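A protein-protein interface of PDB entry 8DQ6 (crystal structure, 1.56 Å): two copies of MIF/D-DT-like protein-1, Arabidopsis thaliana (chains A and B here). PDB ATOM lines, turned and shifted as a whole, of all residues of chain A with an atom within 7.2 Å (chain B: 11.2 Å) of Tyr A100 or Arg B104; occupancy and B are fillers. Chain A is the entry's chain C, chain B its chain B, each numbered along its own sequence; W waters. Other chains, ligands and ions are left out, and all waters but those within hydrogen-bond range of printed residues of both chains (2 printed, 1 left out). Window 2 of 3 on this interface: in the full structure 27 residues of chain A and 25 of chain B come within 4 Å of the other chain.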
ATOM      1  N   LEU A  62      -7.583  17.146 -12.801  1.00  0.00           N
ATOM      2  CA  LEU A  62      -7.263  16.556 -11.507  1.00  0.00           C
ATOM      3  C   LEU A  62      -7.166  15.045 -11.673  1.00  0.00           C
ATOM      4  O   LEU A  62      -8.130  14.404 -12.106  1.00  0.00           O
ATOM      5  CB  LEU A  62      -8.320  16.922 -10.465  1.00  0.00           C
ATOM      6  CG  LEU A  62      -8.446  18.406 -10.123  1.00  0.00           C
ATOM      7  CD1 LEU A  62      -9.772  18.742  -9.454  1.00  0.00           C
ATOM      8  CD2 LEU A  62      -7.306  18.770  -9.193  1.00  0.00           C
ATOM      9  N   SER A  64      -5.933  11.225  -9.966  1.00  0.00           N
ATOM     10  CA  SER A  64      -5.624  10.431  -8.777  1.00  0.00           C
ATOM     11  C   SER A  64      -6.012  11.187  -7.510  1.00  0.00           C
ATOM     12  O   SER A  64      -5.240  11.290  -6.553  1.00  0.00           O
ATOM     13  CB  SER A  64      -4.149  10.014  -8.748  1.00  0.00           C
ATOM     14  OG  SER A  64      -3.792   9.287  -9.914  1.00  0.00           O
ATOM     15  N   ILE A  65      -7.221  11.739  -7.524  1.00  0.00           N
ATOM     16  CA  ILE A  65      -7.802  12.335  -6.329  1.00  0.00           C
ATOM     17  C   ILE A  65      -8.589  11.263  -5.582  1.00  0.00           C
ATOM     18  O   ILE A  65      -8.687  11.287  -4.357  1.00  0.00           O
ATOM     19  CB  ILE A  65      -8.694  13.534  -6.671  1.00  0.00           C
ATOM     20  N   ASN A  73     -13.343  17.901  -4.139  1.00  0.00           N
ATOM     21  CA  ASN A  73     -13.113  18.340  -5.515  1.00  0.00           C
ATOM     22  C   ASN A  73     -13.683  19.732  -5.767  1.00  0.00           C
ATOM     23  O   ASN A  73     -13.082  20.533  -6.494  1.00  0.00           O
ATOM     24  CB  ASN A  73     -13.714  17.333  -6.498  1.00  0.00           C
ATOM     25  CG  ASN A  73     -13.055  15.963  -6.415  1.00  0.00           C
ATOM     26  OD1 ASN A  73     -11.844  15.851  -6.221  1.00  0.00           O
ATOM     27  ND2 ASN A  73     -13.853  14.911  -6.573  1.00  0.00           N
ATOM     28  N   TYR A  96     -11.583  19.541 -14.490  1.00  0.00           N
ATOM     29  CA  TYR A  96     -12.094  18.240 -14.898  1.00  0.00           C
ATOM     30  C   TYR A  96     -11.426  17.144 -14.069  1.00  0.00           C
ATOM     31  O   TYR A  96     -10.195  17.079 -13.994  1.00  0.00           O
ATOM     32  CB  TYR A  96     -11.835  18.039 -16.397  1.00  0.00           C
ATOM     33  CG  TYR A  96     -12.062  16.643 -16.918  1.00  0.00           C
ATOM     34  CD1 TYR A  96     -13.291  16.024 -16.785  1.00  0.00           C
ATOM     35  CD2 TYR A  96     -11.045  15.962 -17.582  1.00  0.00           C
ATOM     36  CE1 TYR A  96     -13.492  14.742 -17.274  1.00  0.00           C
ATOM     37  CE2 TYR A  96     -11.240  14.691 -18.068  1.00  0.00           C
ATOM     38  CZ  TYR A  96     -12.466  14.091 -17.915  1.00  0.00           C
ATOM     39  OH  TYR A  96     -12.670  12.815 -18.403  1.00  0.00           O
ATOM     40  N   ILE A  97     -12.232  16.289 -13.437  1.00  0.00           N
ATOM     41  CA  ILE A  97     -11.725  15.104 -12.746  1.00  0.00           C
ATOM     42  C   ILE A  97     -11.497  14.015 -13.786  1.00  0.00           C
ATOM     43  O   ILE A  97     -12.449  13.520 -14.397  1.00  0.00           O
ATOM     44  CB  ILE A  97     -12.710  14.615 -11.671  1.00  0.00           C
ATOM     45  CG1 ILE A  97     -13.305  15.765 -10.859  1.00  0.00           C
ATOM     46  CG2 ILE A  97     -12.049  13.565 -10.781  1.00  0.00           C
ATOM     47  CD1 ILE A  97     -12.323  16.676 -10.243  1.00  0.00           C
ATOM     48  N   LYS A  98     -10.244  13.617 -13.972  1.00  0.00           N
ATOM     49  CA  LYS A  98      -9.851  12.761 -15.081  1.00  0.00           C
ATOM     50  C   LYS A  98      -9.595  11.338 -14.593  1.00  0.00           C
ATOM     51  O   LYS A  98      -9.047  11.134 -13.504  1.00  0.00           O
ATOM     52  CB  LYS A  98      -8.606  13.345 -15.772  1.00  0.00           C
ATOM     53  CG  LYS A  98      -8.279  12.743 -17.146  1.00  0.00           C
ATOM     54  CD  LYS A  98      -7.095  13.489 -17.786  1.00  0.00           C
ATOM     55  CE  LYS A  98      -7.032  13.267 -19.299  1.00  0.00           C
ATOM     56  NZ  LYS A  98      -5.837  13.953 -19.881  1.00  0.00           N
ATOM     57  N   PHE A  99     -10.026  10.362 -15.398  1.00  0.00           N
ATOM     58  CA  PHE A  99      -9.796   8.931 -15.191  1.00  0.00           C
ATOM     59  C   PHE A  99     -10.562   8.351 -14.007  1.00  0.00           C
ATOM     60  O   PHE A  99     -10.203   7.282 -13.511  1.00  0.00           O
ATOM     61  CB  PHE A  99      -8.307   8.604 -15.015  1.00  0.00           C
ATOM     62  CG  PHE A  99      -7.432   9.104 -16.134  1.00  0.00           C
ATOM     63  CD1 PHE A  99      -7.682   8.742 -17.448  1.00  0.00           C
ATOM     64  CD2 PHE A  99      -6.342   9.919 -15.862  1.00  0.00           C
ATOM     65  CE1 PHE A  99      -6.850   9.192 -18.480  1.00  0.00           C
ATOM     66  CE2 PHE A  99      -5.503  10.369 -16.885  1.00  0.00           C
ATOM     67  CZ  PHE A  99      -5.762  10.013 -18.194  1.00  0.00           C
ATOM     68  N   TYR A 100     -11.612   9.014 -13.539  1.00  0.00           N
ATOM     69  CA  TYR A 100     -12.358   8.497 -12.392  1.00  0.00           C
ATOM     70  C   TYR A 100     -13.742   8.022 -12.816  1.00  0.00           C
ATOM     71  O   TYR A 100     -13.872   6.978 -13.458  1.00  0.00           O
ATOM     72  CB  TYR A 100     -12.466   9.558 -11.295  1.00  0.00           C
ATOM     73  N   PRO B   1     -18.121  21.317 -23.663  1.00  0.00           N
ATOM     74  CA  PRO B   1     -17.025  20.365 -23.839  1.00  0.00           C
ATOM     75  C   PRO B   1     -15.673  21.054 -23.963  1.00  0.00           C
ATOM     76  O   PRO B   1     -15.597  22.255 -24.209  1.00  0.00           O
ATOM     77  CB  PRO B   1     -17.382  19.652 -25.144  1.00  0.00           C
ATOM     78  CG  PRO B   1     -18.138  20.672 -25.906  1.00  0.00           C
ATOM     79  CD  PRO B   1     -18.942  21.431 -24.879  1.00  0.00           C
ATOM     80  N   THR B   2     -14.613  20.268 -23.797  1.00  0.00           N
ATOM     81  CA  THR B   2     -13.247  20.752 -23.931  1.00  0.00           C
ATOM     82  C   THR B   2     -12.525  19.946 -24.997  1.00  0.00           C
ATOM     83  O   THR B   2     -12.575  18.709 -24.994  1.00  0.00           O
ATOM     84  CB  THR B   2     -12.493  20.627 -22.603  1.00  0.00           C
ATOM     85  OG1 THR B   2     -13.156  21.407 -21.609  1.00  0.00           O
ATOM     86  CG2 THR B   2     -11.052  21.123 -22.732  1.00  0.00           C
ATOM     87  N   ILE B  63     -13.298  16.102 -24.371  1.00  0.00           N
ATOM     88  CA  ILE B  63     -13.930  15.761 -23.105  1.00  0.00           C
ATOM     89  C   ILE B  63     -15.345  16.322 -23.129  1.00  0.00           C
ATOM     90  O   ILE B  63     -15.539  17.542 -23.210  1.00  0.00           O
ATOM     91  CB  ILE B  63     -13.134  16.310 -21.916  1.00  0.00           C
ATOM     92  CG1 ILE B  63     -11.702  15.759 -21.932  1.00  0.00           C
ATOM     93  CG2 ILE B  63     -13.831  15.936 -20.623  1.00  0.00           C
ATOM     94  CD1 ILE B  63     -10.671  16.816 -22.210  1.00  0.00           C
ATOM     95  N   SER B  64     -16.335  15.432 -23.085  1.00  0.00           N
ATOM     96  CA  SER B  64     -17.730  15.830 -23.000  1.00  0.00           C
ATOM     97  C   SER B  64     -18.314  15.263 -21.721  1.00  0.00           C
ATOM     98  O   SER B  64     -17.913  14.192 -21.252  1.00  0.00           O
ATOM     99  CB  SER B  64     -18.539  15.340 -24.195  1.00  0.00           C
ATOM    100  OG  SER B  64     -18.587  13.926 -24.204  1.00  0.00           O
ATOM    101  N   ILE B  65     -19.256  15.997 -21.149  1.00  0.00           N
ATOM    102  CA  ILE B  65     -19.964  15.526 -19.965  1.00  0.00           C
ATOM    103  C   ILE B  65     -21.039  14.555 -20.444  1.00  0.00           C
ATOM    104  O   ILE B  65     -21.985  14.955 -21.120  1.00  0.00           O
ATOM    105  CB  ILE B  65     -20.566  16.692 -19.175  1.00  0.00           C
ATOM    106  CG1 ILE B  65     -19.475  17.720 -18.838  1.00  0.00           C
ATOM    107  CG2 ILE B  65     -21.213  16.191 -17.898  1.00  0.00           C
ATOM    108  CD1 ILE B  65     -18.136  17.111 -18.385  1.00  0.00           C
ATOM    109  N   GLY B  66     -20.865  13.269 -20.144  1.00  0.00           N
ATOM    110  CA  GLY B  66     -21.850  12.259 -20.489  1.00  0.00           C
ATOM    111  C   GLY B  66     -21.728  11.639 -21.870  1.00  0.00           C
ATOM    112  O   GLY B  66     -22.533  10.761 -22.212  1.00  0.00           O
ATOM    113  N   GLY B  67     -20.772  12.063 -22.681  1.00  0.00           N
ATOM    114  CA  GLY B  67     -20.561  11.445 -23.971  1.00  0.00           C
ATOM    115  C   GLY B  67     -21.567  11.884 -25.018  1.00  0.00           C
ATOM    116  O   GLY B  67     -22.556  12.576 -24.750  1.00  0.00           O
ATOM    117  N   LYS B  98      -8.840  11.171 -28.856  1.00  0.00           N
ATOM    118  CA  LYS B  98      -9.418  10.333 -27.818  1.00  0.00           C
ATOM    119  C   LYS B  98     -10.603  11.069 -27.212  1.00  0.00           C
ATOM    120  O   LYS B  98     -10.508  12.261 -26.884  1.00  0.00           O
ATOM    121  CB  LYS B  98      -8.381   9.979 -26.744  1.00  0.00           C
ATOM    122  CG  LYS B  98      -8.755   8.749 -25.920  1.00  0.00           C
ATOM    123  CD  LYS B  98      -9.168   9.164 -24.548  1.00  0.00           C
ATOM    124  CE  LYS B  98      -9.454   7.986 -23.636  1.00  0.00           C
ATOM    125  NZ  LYS B  98     -10.857   7.524 -23.798  1.00  0.00           N
ATOM    126  N   TYR B 100     -13.391  11.396 -24.156  1.00  0.00           N
ATOM    127  CA  TYR B 100     -13.659  11.128 -22.746  1.00  0.00           C
ATOM    128  C   TYR B 100     -15.123  11.420 -22.473  1.00  0.00           C
ATOM    129  O   TYR B 100     -15.574  12.550 -22.678  1.00  0.00           O
ATOM    130  CB  TYR B 100     -12.807  12.001 -21.827  1.00  0.00           C
ATOM    131  CG  TYR B 100     -11.332  11.716 -21.810  1.00  0.00           C
ATOM    132  CD1 TYR B 100     -10.767  10.984 -20.772  1.00  0.00           C
ATOM    133  CD2 TYR B 100     -10.500  12.196 -22.813  1.00  0.00           C
ATOM    134  CE1 TYR B 100      -9.415  10.728 -20.736  1.00  0.00           C
ATOM    135  CE2 TYR B 100      -9.139  11.953 -22.782  1.00  0.00           C
ATOM    136  CZ  TYR B 100      -8.612  11.206 -21.745  1.00  0.00           C
ATOM    137  OH  TYR B 100      -7.281  10.946 -21.684  1.00  0.00           O
ATOM    138  N   ASP B 101     -15.847  10.428 -21.964  1.00  0.00           N
ATOM    139  CA  ASP B 101     -17.247  10.615 -21.584  1.00  0.00           C
ATOM    140  C   ASP B 101     -17.295  10.792 -20.066  1.00  0.00           C
ATOM    141  O   ASP B 101     -17.293   9.815 -19.315  1.00  0.00           O
ATOM    142  CB  ASP B 101     -18.094   9.441 -22.061  1.00  0.00           C
ATOM    143  CG  ASP B 101     -18.003   9.227 -23.571  1.00  0.00           C
ATOM    144  OD1 ASP B 101     -17.538  10.145 -24.287  1.00  0.00           O
ATOM    145  OD2 ASP B 101     -18.397   8.139 -24.044  1.00  0.00           O
ATOM    146  N   SER B 102     -17.312  12.041 -19.614  1.00  0.00           N
ATOM    147  CA  SER B 102     -17.212  12.309 -18.183  1.00  0.00           C
ATOM    148  C   SER B 102     -18.537  11.984 -17.507  1.00  0.00           C
ATOM    149  O   SER B 102     -19.580  12.505 -17.915  1.00  0.00           O
ATOM    150  CB  SER B 102     -16.831  13.766 -17.921  1.00  0.00           C
ATOM    151  OG  SER B 102     -16.925  14.087 -16.535  1.00  0.00           O
ATOM    152  N   PRO B 103     -18.541  11.139 -16.475  1.00  0.00           N
ATOM    153  CA  PRO B 103     -19.790  10.833 -15.772  1.00  0.00           C
ATOM    154  C   PRO B 103     -20.215  11.892 -14.767  1.00  0.00           C
ATOM    155  O   PRO B 103     -21.255  11.722 -14.121  1.00  0.00           O
ATOM    156  CB  PRO B 103     -19.465   9.508 -15.069  1.00  0.00           C
ATOM    157  CG  PRO B 103     -17.979   9.585 -14.802  1.00  0.00           C
ATOM    158  CD  PRO B 103     -17.374  10.454 -15.884  1.00  0.00           C
ATOM    159  N   ARG B 104     -19.458  12.971 -14.615  1.00  0.00           N
ATOM    160  CA  ARG B 104     -19.768  14.020 -13.656  1.00  0.00           C
ATOM    161  C   ARG B 104     -19.423  15.363 -14.280  1.00  0.00           C
ATOM    162  O   ARG B 104     -18.608  15.430 -15.208  1.00  0.00           O
ATOM    163  CB  ARG B 104     -19.004  13.818 -12.337  1.00  0.00           C
ATOM    164  CG  ARG B 104     -17.503  14.037 -12.439  1.00  0.00           C
ATOM    165  CD  ARG B 104     -16.762  13.573 -11.182  1.00  0.00           C
ATOM    166  NE  ARG B 104     -16.885  12.135 -10.943  1.00  0.00           N
ATOM    167  CZ  ARG B 104     -16.256  11.194 -11.645  1.00  0.00           C
ATOM    168  NH1 ARG B 104     -15.450  11.530 -12.642  1.00  0.00           N
ATOM    169  NH2 ARG B 104     -16.434   9.909 -11.350  1.00  0.00           N
ATOM    170  N   PRO B 105     -20.040  16.444 -13.810  1.00  0.00           N
ATOM    171  CA  PRO B 105     -19.845  17.744 -14.465  1.00  0.00           C
ATOM    172  C   PRO B 105     -18.447  18.307 -14.241  1.00  0.00           C
ATOM    173  O   PRO B 105     -17.708  17.895 -13.342  1.00  0.00           O
ATOM    174  CB  PRO B 105     -20.905  18.638 -13.813  1.00  0.00           C
ATOM    175  CG  PRO B 105     -21.921  17.673 -13.212  1.00  0.00           C
ATOM    176  CD  PRO B 105     -21.105  16.493 -12.790  1.00  0.00           C
ATOM    177  N   PHE B 106     -18.084  19.261 -15.100  1.00  0.00           N
ATOM    178  CA  PHE B 106     -16.937  20.115 -14.826  1.00  0.00           C
ATOM    179  C   PHE B 106     -17.212  20.971 -13.595  1.00  0.00           C
ATOM    180  O   PHE B 106     -18.360  21.191 -13.195  1.00  0.00           O
ATOM    181  CB  PHE B 106     -16.636  21.065 -15.995  1.00  0.00           C
ATOM    182  CG  PHE B 106     -16.263  20.382 -17.290  1.00  0.00           C
ATOM    183  CD1 PHE B 106     -15.178  19.523 -17.359  1.00  0.00           C
ATOM    184  CD2 PHE B 106     -16.982  20.638 -18.453  1.00  0.00           C
ATOM    185  CE1 PHE B 106     -14.837  18.908 -18.558  1.00  0.00           C
ATOM    186  CE2 PHE B 106     -16.649  20.027 -19.652  1.00  0.00           C
ATOM    187  CZ  PHE B 106     -15.580  19.164 -19.710  1.00  0.00           C
ATOM    188  N   PHE B 107     -16.142  21.473 -13.000  1.00  0.00           N
ATOM    189  CA  PHE B 107     -16.224  22.546 -12.018  1.00  0.00           C
ATOM    190  C   PHE B 107     -15.798  23.820 -12.730  1.00  0.00           C
ATOM    191  O   PHE B 107     -14.627  23.963 -13.098  1.00  0.00           O
ATOM    192  CB  PHE B 107     -15.330  22.262 -10.814  1.00  0.00           C
ATOM    193  CG  PHE B 107     -15.717  21.035 -10.054  1.00  0.00           C
ATOM    194  CD1 PHE B 107     -16.670  21.105  -9.048  1.00  0.00           C
ATOM    195  CD2 PHE B 107     -15.132  19.812 -10.343  1.00  0.00           C
ATOM    196  CE1 PHE B 107     -17.031  19.967  -8.344  1.00  0.00           C
ATOM    197  CE2 PHE B 107     -15.488  18.675  -9.639  1.00  0.00           C
ATOM    198  CZ  PHE B 107     -16.439  18.753  -8.640  1.00  0.00           C
ATOM    199  N   GLY B 108     -16.743  24.729 -12.947  1.00  0.00           N
ATOM    200  CA  GLY B 108     -16.480  25.945 -13.686  1.00  0.00           C
ATOM    201  C   GLY B 108     -16.678  27.164 -12.807  1.00  0.00           C
ATOM    202  O   GLY B 108     -17.520  27.166 -11.905  1.00  0.00           O
HETATM  203  O   HOH W   1     -15.113  16.595 -13.774  1.00  0.00           O
HETATM  204  O   HOH W   2     -14.987  13.862 -14.261  1.00  0.00           O
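Water W2 lies within hydrogen-bond range of the backbone carbonyl oxygen of Ile A97 (2.6 Å), the guanidinium group of Arg B104 (2.9 Å) and the side-chain hydroxyl of Ser B102 (3.0 Å). Water W1 lies within hydrogen-bond range of the backbone NH of Ile A97 (2.9 Å) and the backbone carbonyl oxygen of Pro B105 (2.9 Å).
Among the printed residues, pairs that only touch across the chains: Asn A73 with Phe B107 (3.7 Å), Tyr A96 with Ile B63 (3.5 Å), Tyr A96 with Tyr B100 (3.5 Å), Tyr A96 with Ser B102 (3.5 Å), Tyr A96 with Phe B106 (3.7 Å), Ile A97 with Phe B107 (3.8 Å), Lys A98 with Tyr B100 (3.3 Å), Phe A99 with Tyr B100 (3.7 Å) and Tyr A100 with Arg B104 (3.6 Å).
Of chain B, only Arg B104 comes within 4 Å of Tyr A100. Gly B67 touches none of the printed residues of chain A. Of the printed residues of chain A, Ser B102 touches Tyr A96 (3.5 Å). Printed residues of chain A within 4 Å of Arg B104: Tyr A100. Printed residues of chain A within 4 Å of Phe B107: Asn A73 and Ile A97. Gly B108 touches none of the printed residues of chain A. The nearest residue of chain B that does not touch Tyr A100 is Pro B103 (4.9 Å). The nearest printed residue of chain A that does not touch Arg B104 is Ile A97 (4.01 Å).
Lys A98 touches Tyr B100, but with the chains exchanged Tyr A100 does not touch Lys B98 (10.4 Å). 4 positions are printed for both chains. Of the 9 pairs that touch across the chains among the printed residues, none has its exchanged pair printed and touching as well.
Of the 9 printed residues of chain A, 6 touch a printed residue of chain B. Printed residues of chain A that touch a printed residue of chain B: Asn A73, Tyr A96, Ile A97, Lys A98, Phe A99 and Tyr A100. Hydrophobic or aromatic side chains of chain A that line the printed part of chain B: Tyr A96, Ile A97, Phe A99 and Tyr A100. Among the printed residues, 9 pairs touch across the chains.
The backbone carbonyl oxygen of Thr B2 lies within hydrogen-bond range of the backbone NH of Ile B63 (2.8 Å). The backbone NH (N) of Ser B64 sits at hydrogen-bond distance from the backbone carbonyl oxygen (O) of Tyr B100 (3.0 Å). O of Ser B64 lies within hydrogen-bond range of N of Ser B102, 2.8 Å away. N of Gly B66 is in hydrogen-bond range of O of Ser B102 (2.7 Å). The side-chain hydroxyl (OG) of Ser B102 lies within hydrogen-bond range of the backbone carbonyl oxygen (O) of Arg B104, 2.5 Å away. The backbone NH (N) of Lys A98 is in hydrogen-bond range of the backbone carbonyl oxygen (O) of Leu A62.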
